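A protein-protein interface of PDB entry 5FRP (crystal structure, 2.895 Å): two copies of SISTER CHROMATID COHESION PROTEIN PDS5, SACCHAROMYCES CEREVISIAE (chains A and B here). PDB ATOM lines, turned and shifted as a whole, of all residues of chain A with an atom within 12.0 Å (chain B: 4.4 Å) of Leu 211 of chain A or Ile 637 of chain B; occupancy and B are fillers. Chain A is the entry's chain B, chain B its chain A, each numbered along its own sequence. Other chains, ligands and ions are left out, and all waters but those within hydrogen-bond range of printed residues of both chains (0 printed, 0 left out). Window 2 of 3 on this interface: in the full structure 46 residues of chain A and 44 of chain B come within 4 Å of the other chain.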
ATOM      1  N   ALA A 167       1.243  14.996 -11.081  1.00  0.00           N
ATOM      2  CA  ALA A 167       2.213  13.930 -10.862  1.00  0.00           C
ATOM      3  C   ALA A 167       1.598  12.534 -10.948  1.00  0.00           C
ATOM      4  O   ALA A 167       2.252  11.595 -11.401  1.00  0.00           O
ATOM      5  CB  ALA A 167       2.884  14.118  -9.511  1.00  0.00           C
ATOM      6  N   TYR A 202      17.948  18.625 -17.224  1.00  0.00           N
ATOM      7  CA  TYR A 202      17.322  18.542 -15.909  1.00  0.00           C
ATOM      8  C   TYR A 202      18.110  17.609 -14.999  1.00  0.00           C
ATOM      9  O   TYR A 202      18.034  16.389 -15.140  1.00  0.00           O
ATOM     10  CB  TYR A 202      15.873  18.069 -16.034  1.00  0.00           C
ATOM     11  CG  TYR A 202      15.180  17.876 -14.703  1.00  0.00           C
ATOM     12  CD1 TYR A 202      15.235  16.658 -14.037  1.00  0.00           C
ATOM     13  CD2 TYR A 202      14.468  18.913 -14.115  1.00  0.00           C
ATOM     14  CE1 TYR A 202      14.602  16.478 -12.820  1.00  0.00           C
ATOM     15  CE2 TYR A 202      13.829  18.744 -12.900  1.00  0.00           C
ATOM     16  CZ  TYR A 202      13.901  17.525 -12.259  1.00  0.00           C
ATOM     17  OH  TYR A 202      13.268  17.349 -11.049  1.00  0.00           O
ATOM     18  N   PRO A 204      18.446  16.385 -11.191  1.00  0.00           N
ATOM     19  CA  PRO A 204      17.764  16.447  -9.890  1.00  0.00           C
ATOM     20  C   PRO A 204      18.632  16.863  -8.698  1.00  0.00           C
ATOM     21  O   PRO A 204      18.109  16.902  -7.584  1.00  0.00           O
ATOM     22  CB  PRO A 204      17.269  15.009  -9.688  1.00  0.00           C
ATOM     23  CG  PRO A 204      17.226  14.415 -11.044  1.00  0.00           C
ATOM     24  CD  PRO A 204      18.355  15.041 -11.790  1.00  0.00           C
ATOM     25  N   ASN A 205      19.910  17.165  -8.909  1.00  0.00           N
ATOM     26  CA  ASN A 205      20.753  17.640  -7.815  1.00  0.00           C
ATOM     27  C   ASN A 205      21.071  19.130  -7.956  1.00  0.00           C
ATOM     28  O   ASN A 205      21.813  19.688  -7.148  1.00  0.00           O
ATOM     29  CB  ASN A 205      22.041  16.811  -7.741  1.00  0.00           C
ATOM     30  CG  ASN A 205      22.970  17.032  -8.927  1.00  0.00           C
ATOM     31  OD1 ASN A 205      23.264  18.165  -9.305  1.00  0.00           O
ATOM     32  ND2 ASN A 205      23.427  15.938  -9.525  1.00  0.00           N
ATOM     33  N   GLU A 206      20.510  19.762  -8.982  1.00  0.00           N
ATOM     34  CA  GLU A 206      20.691  21.193  -9.214  1.00  0.00           C
ATOM     35  C   GLU A 206      19.560  22.003  -8.574  1.00  0.00           C
ATOM     36  O   GLU A 206      19.741  23.171  -8.235  1.00  0.00           O
ATOM     37  CB  GLU A 206      20.795  21.502 -10.713  1.00  0.00           C
ATOM     38  CG  GLU A 206      19.469  21.704 -11.430  1.00  0.00           C
ATOM     39  CD  GLU A 206      19.635  21.952 -12.917  1.00  0.00           C
ATOM     40  OE1 GLU A 206      20.714  22.421 -13.334  1.00  0.00           O
ATOM     41  OE2 GLU A 206      18.678  21.677 -13.672  1.00  0.00           O
ATOM     42  N   ILE A 207      18.402  21.366  -8.416  1.00  0.00           N
ATOM     43  CA  ILE A 207      17.171  22.047  -8.025  1.00  0.00           C
ATOM     44  C   ILE A 207      16.816  21.890  -6.531  1.00  0.00           C
ATOM     45  O   ILE A 207      15.929  22.585  -6.033  1.00  0.00           O
ATOM     46  CB  ILE A 207      15.984  21.547  -8.914  1.00  0.00           C
ATOM     47  CG1 ILE A 207      16.105  22.139 -10.324  1.00  0.00           C
ATOM     48  CG2 ILE A 207      14.624  21.886  -8.278  1.00  0.00           C
ATOM     49  CD1 ILE A 207      14.956  21.789 -11.258  1.00  0.00           C
ATOM     50  N   PRO A 208      17.524  21.026  -5.781  1.00  0.00           N
ATOM     51  CA  PRO A 208      17.124  21.068  -4.367  1.00  0.00           C
ATOM     52  C   PRO A 208      17.472  22.372  -3.649  1.00  0.00           C
ATOM     53  O   PRO A 208      18.612  22.833  -3.707  1.00  0.00           O
ATOM     54  CB  PRO A 208      17.901  19.901  -3.749  1.00  0.00           C
ATOM     55  CG  PRO A 208      18.160  18.974  -4.875  1.00  0.00           C
ATOM     56  CD  PRO A 208      18.350  19.841  -6.081  1.00  0.00           C
ATOM     57  N   GLU A 209      16.479  22.953  -2.980  1.00  0.00           N
ATOM     58  CA  GLU A 209      16.663  24.212  -2.265  1.00  0.00           C
ATOM     59  C   GLU A 209      15.478  24.520  -1.346  1.00  0.00           C
ATOM     60  O   GLU A 209      14.772  25.509  -1.547  1.00  0.00           O
ATOM     61  CB  GLU A 209      16.882  25.364  -3.251  1.00  0.00           C
ATOM     62  CG  GLU A 209      15.830  25.475  -4.347  1.00  0.00           C
ATOM     63  CD  GLU A 209      16.221  26.452  -5.440  1.00  0.00           C
ATOM     64  OE1 GLU A 209      17.240  27.156  -5.284  1.00  0.00           O
ATOM     65  OE2 GLU A 209      15.507  26.509  -6.463  1.00  0.00           O
ATOM     66  N   GLY A 210      15.271  23.672  -0.340  1.00  0.00           N
ATOM     67  CA  GLY A 210      14.199  23.866   0.624  1.00  0.00           C
ATOM     68  C   GLY A 210      13.435  22.600   0.970  1.00  0.00           C
ATOM     69  O   GLY A 210      13.700  21.968   1.993  1.00  0.00           O
ATOM     70  N   LEU A 211      12.483  22.232   0.117  1.00  0.00           N
ATOM     71  CA  LEU A 211      11.569  21.123   0.395  1.00  0.00           C
ATOM     72  C   LEU A 211      11.644  20.028  -0.669  1.00  0.00           C
ATOM     73  O   LEU A 211      11.194  18.906  -0.437  1.00  0.00           O
ATOM     74  CB  LEU A 211      10.127  21.613   0.528  1.00  0.00           C
ATOM     75  CG  LEU A 211       9.739  22.129   1.916  1.00  0.00           C
ATOM     76  CD1 LEU A 211      10.167  23.577   2.144  1.00  0.00           C
ATOM     77  CD2 LEU A 211       8.240  21.956   2.141  1.00  0.00           C
ATOM     78  N   ASN A 212      12.193  20.355  -1.836  1.00  0.00           N
ATOM     79  CA  ASN A 212      12.291  19.395  -2.933  1.00  0.00           C
ATOM     80  C   ASN A 212      10.922  18.903  -3.397  1.00  0.00           C
ATOM     81  O   ASN A 212      10.783  17.756  -3.823  1.00  0.00           O
ATOM     82  CB  ASN A 212      13.152  18.190  -2.521  1.00  0.00           C
ATOM     83  CG  ASN A 212      14.626  18.406  -2.779  1.00  0.00           C
ATOM     84  OD1 ASN A 212      15.006  19.070  -3.740  1.00  0.00           O
ATOM     85  ND2 ASN A 212      15.467  17.844  -1.918  1.00  0.00           N
ATOM     86  N   VAL A 213       9.913  19.765  -3.323  1.00  0.00           N
ATOM     87  CA  VAL A 213       8.571  19.371  -3.726  1.00  0.00           C
ATOM     88  C   VAL A 213       8.495  19.335  -5.253  1.00  0.00           C
ATOM     89  O   VAL A 213       7.563  18.764  -5.820  1.00  0.00           O
ATOM     90  CB  VAL A 213       7.506  20.326  -3.137  1.00  0.00           C
ATOM     91  CG1 VAL A 213       7.710  21.762  -3.619  1.00  0.00           C
ATOM     92  CG2 VAL A 213       6.097  19.840  -3.462  1.00  0.00           C
ATOM     93  N   THR A 214       9.483  19.933  -5.912  1.00  0.00           N
ATOM     94  CA  THR A 214       9.488  20.031  -7.367  1.00  0.00           C
ATOM     95  C   THR A 214       9.491  18.646  -8.009  1.00  0.00           C
ATOM     96  O   THR A 214      10.030  17.693  -7.444  1.00  0.00           O
ATOM     97  CB  THR A 214      10.702  20.842  -7.861  1.00  0.00           C
ATOM     98  OG1 THR A 214      10.741  22.092  -7.161  1.00  0.00           O
ATOM     99  CG2 THR A 214      10.610  21.116  -9.358  1.00  0.00           C
ATOM    100  N   SER A 215       8.889  18.550  -9.188  1.00  0.00           N
ATOM    101  CA  SER A 215       8.964  17.350 -10.011  1.00  0.00           C
ATOM    102  C   SER A 215       8.719  17.749 -11.460  1.00  0.00           C
ATOM    103  O   SER A 215       8.203  18.833 -11.728  1.00  0.00           O
ATOM    104  CB  SER A 215       7.941  16.310  -9.556  1.00  0.00           C
ATOM    105  OG  SER A 215       8.211  15.052 -10.153  1.00  0.00           O
ATOM    106  N   SER B 472       5.029  25.815   0.674  1.00  0.00           N
ATOM    107  CA  SER B 472       6.395  25.521   1.090  1.00  0.00           C
ATOM    108  C   SER B 472       7.244  26.784   1.228  1.00  0.00           C
ATOM    109  O   SER B 472       7.983  26.941   2.199  1.00  0.00           O
ATOM    110  CB  SER B 472       7.062  24.568   0.096  1.00  0.00           C
ATOM    111  OG  SER B 472       7.216  25.181  -1.169  1.00  0.00           O
ATOM    112  N   GLU B 476       9.046  29.144   4.528  1.00  0.00           N
ATOM    113  CA  GLU B 476      10.487  28.930   4.461  1.00  0.00           C
ATOM    114  C   GLU B 476      11.252  30.245   4.544  1.00  0.00           C
ATOM    115  O   GLU B 476      12.292  30.321   5.198  1.00  0.00           O
ATOM    116  CB  GLU B 476      10.861  28.197   3.171  1.00  0.00           C
ATOM    117  CG  GLU B 476      11.043  26.697   3.340  1.00  0.00           C
ATOM    118  CD  GLU B 476      12.431  26.310   3.812  1.00  0.00           C
ATOM    119  OE1 GLU B 476      13.427  26.778   3.221  1.00  0.00           O
ATOM    120  OE2 GLU B 476      12.529  25.533   4.786  1.00  0.00           O
ATOM    121  N   LEU B 560      -3.589  17.799  -2.717  1.00  0.00           N
ATOM    122  CA  LEU B 560      -2.187  17.554  -3.041  1.00  0.00           C
ATOM    123  C   LEU B 560      -2.011  17.140  -4.500  1.00  0.00           C
ATOM    124  O   LEU B 560      -2.866  16.459  -5.066  1.00  0.00           O
ATOM    125  CB  LEU B 560      -1.608  16.482  -2.113  1.00  0.00           C
ATOM    126  CG  LEU B 560      -1.810  16.738  -0.614  1.00  0.00           C
ATOM    127  CD1 LEU B 560      -1.006  15.743   0.192  1.00  0.00           C
ATOM    128  CD2 LEU B 560      -1.416  18.160  -0.247  1.00  0.00           C
ATOM    129  N   LYS B 633       7.901  14.851   2.629  1.00  0.00           N
ATOM    130  CA  LYS B 633       7.583  16.013   1.803  1.00  0.00           C
ATOM    131  C   LYS B 633       6.073  16.162   1.621  1.00  0.00           C
ATOM    132  O   LYS B 633       5.595  17.220   1.211  1.00  0.00           O
ATOM    133  CB  LYS B 633       8.297  15.943   0.445  1.00  0.00           C
ATOM    134  CG  LYS B 633       7.677  15.018  -0.588  1.00  0.00           C
ATOM    135  CD  LYS B 633       8.539  14.905  -1.845  1.00  0.00           C
ATOM    136  CE  LYS B 633       9.844  14.157  -1.595  1.00  0.00           C
ATOM    137  NZ  LYS B 633      10.620  13.970  -2.850  1.00  0.00           N
ATOM    138  N   VAL B 634       5.324  15.105   1.924  1.00  0.00           N
ATOM    139  CA  VAL B 634       3.867  15.167   1.854  1.00  0.00           C
ATOM    140  C   VAL B 634       3.317  15.729   3.165  1.00  0.00           C
ATOM    141  O   VAL B 634       2.538  16.687   3.161  1.00  0.00           O
ATOM    142  CB  VAL B 634       3.255  13.778   1.562  1.00  0.00           C
ATOM    143  CG1 VAL B 634       1.734  13.818   1.671  1.00  0.00           C
ATOM    144  CG2 VAL B 634       3.675  13.296   0.182  1.00  0.00           C
ATOM    145  N   ILE B 635       3.719  15.140   4.285  1.00  0.00           N
ATOM    146  CA  ILE B 635       3.141  15.511   5.567  1.00  0.00           C
ATOM    147  C   ILE B 635       3.596  16.913   5.953  1.00  0.00           C
ATOM    148  O   ILE B 635       2.887  17.621   6.663  1.00  0.00           O
ATOM    149  CB  ILE B 635       3.502  14.491   6.662  1.00  0.00           C
ATOM    150  CG1 ILE B 635       2.668  14.747   7.922  1.00  0.00           C
ATOM    151  CG2 ILE B 635       5.000  14.512   6.971  1.00  0.00           C
ATOM    152  CD1 ILE B 635       2.824  13.682   8.984  1.00  0.00           C
ATOM    153  N   GLN B 636       4.783  17.311   5.504  1.00  0.00           N
ATOM    154  CA  GLN B 636       5.295  18.644   5.816  1.00  0.00           C
ATOM    155  C   GLN B 636       4.414  19.721   5.183  1.00  0.00           C
ATOM    156  O   GLN B 636       3.838  20.568   5.885  1.00  0.00           O
ATOM    157  CB  GLN B 636       6.738  18.776   5.328  1.00  0.00           C
ATOM    158  CG  GLN B 636       7.253  20.200   5.270  1.00  0.00           C
ATOM    159  CD  GLN B 636       8.765  20.258   5.156  1.00  0.00           C
ATOM    160  OE1 GLN B 636       9.425  19.228   5.020  1.00  0.00           O
ATOM    161  NE2 GLN B 636       9.319  21.462   5.213  1.00  0.00           N
ATOM    162  N   ILE B 637       4.307  19.674   3.859  1.00  0.00           N
ATOM    163  CA  ILE B 637       3.445  20.589   3.129  1.00  0.00           C
ATOM    164  C   ILE B 637       2.019  20.451   3.638  1.00  0.00           C
ATOM    165  O   ILE B 637       1.283  21.436   3.706  1.00  0.00           O
ATOM    166  CB  ILE B 637       3.526  20.375   1.597  1.00  0.00           C
ATOM    167  CG1 ILE B 637       3.190  18.940   1.187  1.00  0.00           C
ATOM    168  CG2 ILE B 637       4.927  20.713   1.105  1.00  0.00           C
ATOM    169  CD1 ILE B 637       1.748  18.694   0.822  1.00  0.00           C
ATOM    170  N   LEU B 638       1.626  19.230   3.988  1.00  0.00           N
ATOM    171  CA  LEU B 638       0.288  19.001   4.516  1.00  0.00           C
ATOM    172  C   LEU B 638       0.122  19.728   5.853  1.00  0.00           C
ATOM    173  O   LEU B 638      -0.932  20.299   6.127  1.00  0.00           O
ATOM    174  CB  LEU B 638       0.027  17.505   4.682  1.00  0.00           C
ATOM    175  CG  LEU B 638      -1.405  17.099   5.037  1.00  0.00           C
ATOM    176  CD1 LEU B 638      -2.359  17.417   3.896  1.00  0.00           C
ATOM    177  CD2 LEU B 638      -1.452  15.620   5.378  1.00  0.00           C
ATOM    178  N   LEU B 639       1.164  19.699   6.683  1.00  0.00           N
ATOM    179  CA  LEU B 639       1.137  20.371   7.983  1.00  0.00           C
ATOM    180  C   LEU B 639       1.125  21.886   7.849  1.00  0.00           C
ATOM    181  O   LEU B 639       0.436  22.570   8.608  1.00  0.00           O
ATOM    182  CB  LEU B 639       2.328  19.942   8.846  1.00  0.00           C
ATOM    183  CG  LEU B 639       2.100  18.746   9.777  1.00  0.00           C
ATOM    184  CD1 LEU B 639       3.405  18.363  10.450  1.00  0.00           C
ATOM    185  CD2 LEU B 639       1.032  19.063  10.822  1.00  0.00           C
ATOM    186  N   PHE B 640       1.891  22.414   6.897  1.00  0.00           N
ATOM    187  CA  PHE B 640       1.908  23.860   6.673  1.00  0.00           C
ATOM    188  C   PHE B 640       0.497  24.437   6.547  1.00  0.00           C
ATOM    189  O   PHE B 640       0.266  25.593   6.898  1.00  0.00           O
ATOM    190  CB  PHE B 640       2.710  24.221   5.418  1.00  0.00           C
ATOM    191  CG  PHE B 640       4.206  24.086   5.555  1.00  0.00           C
ATOM    192  CD1 PHE B 640       4.807  23.873   6.786  1.00  0.00           C
ATOM    193  CD2 PHE B 640       5.013  24.190   4.435  1.00  0.00           C
ATOM    194  CE1 PHE B 640       6.180  23.760   6.894  1.00  0.00           C
ATOM    195  CE2 PHE B 640       6.385  24.078   4.536  1.00  0.00           C
ATOM    196  CZ  PHE B 640       6.970  23.863   5.768  1.00  0.00           C
ATOM    197  N   ARG B 641      -0.441  23.635   6.052  1.00  0.00           N
ATOM    198  CA  ARG B 641      -1.832  24.067   5.944  1.00  0.00           C
ATOM    199  C   ARG B 641      -2.636  23.697   7.191  1.00  0.00           C
ATOM    200  O   ARG B 641      -3.658  24.319   7.481  1.00  0.00           O
ATOM    201  CB  ARG B 641      -2.497  23.445   4.713  1.00  0.00           C
ATOM    202  CG  ARG B 641      -1.644  23.508   3.456  1.00  0.00           C
ATOM    203  CD  ARG B 641      -2.391  22.923   2.266  1.00  0.00           C
ATOM    204  NE  ARG B 641      -1.542  22.870   1.079  1.00  0.00           N
ATOM    205  CZ  ARG B 641      -1.973  22.565  -0.141  1.00  0.00           C
ATOM    206  NH1 ARG B 641      -3.257  22.288  -0.336  1.00  0.00           N
ATOM    207  NH2 ARG B 641      -1.130  22.536  -1.163  1.00  0.00           N
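Among the printed residues, pairs that only touch across the chains: Leu 211 of chain A with Gln 636 of chain B, Leu 211 of chain A with Glu 476 of chain B, Leu 211 of chain A with Ser 472 of chain B, Leu 211 of chain A with Ile 637 of chain B, Leu 211 of chain A with Phe 640 of chain B, Asn 212 of chain A with Lys 633 of chain B and Gly 210 of chain A with Glu 476 of chain B.
Ile 207 of chain A touches none of the printed residues of chain B. Pro 208 of chain A touches none of the printed residues of chain B. Printed residues of chain B within 4 Å of Gly 210 of chain A: Glu 476. Of chain B, only Ser 472, Glu 476, Gln 636, Ile 637 and Phe 640 come within 4 Å of Leu 211 of chain A. Printed residues of chain B within 4 Å of Asn 212 of chain A: Lys 633. Of the printed residues of chain A, Ser 472 of chain B touches Leu 211. No residue of chain A comes within 4 Å of Leu 560 of chain B. Of chain A, only Asn 212 comes within 4 Å of Lys 633 of chain B. No residue of chain A comes within 4 Å of Val 634 of chain B. Of chain A, only Leu 211 (3.7 Å) comes within 4 Å of Ile 637 of chain B. No residue of chain A comes within 4 Å of Leu 638 of chain B. No residue of chain A comes within 4 Å of Leu 639 of chain B. Of chain A, only Leu 211 (3.7 Å) comes within 4 Å of Phe 640 of chain B. The nearest residue of chain B that does not touch Leu 211 of chain A is Lys 633 of chain B (4.2 Å).
Of the 12 printed residues of chain B, 6 touch a printed residue of chain A. Printed residues of chain B that touch a printed residue of chain A: Ser 472, Glu 476, Lys 633, Gln 636, Ile 637 and Phe 640. Of the 14 printed residues of chain A, 3 touch a printed residue of chain B. Hydrophobic or aromatic side chains of chain A that line the printed part of chain B: Leu 211.
No position is printed for both chains.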
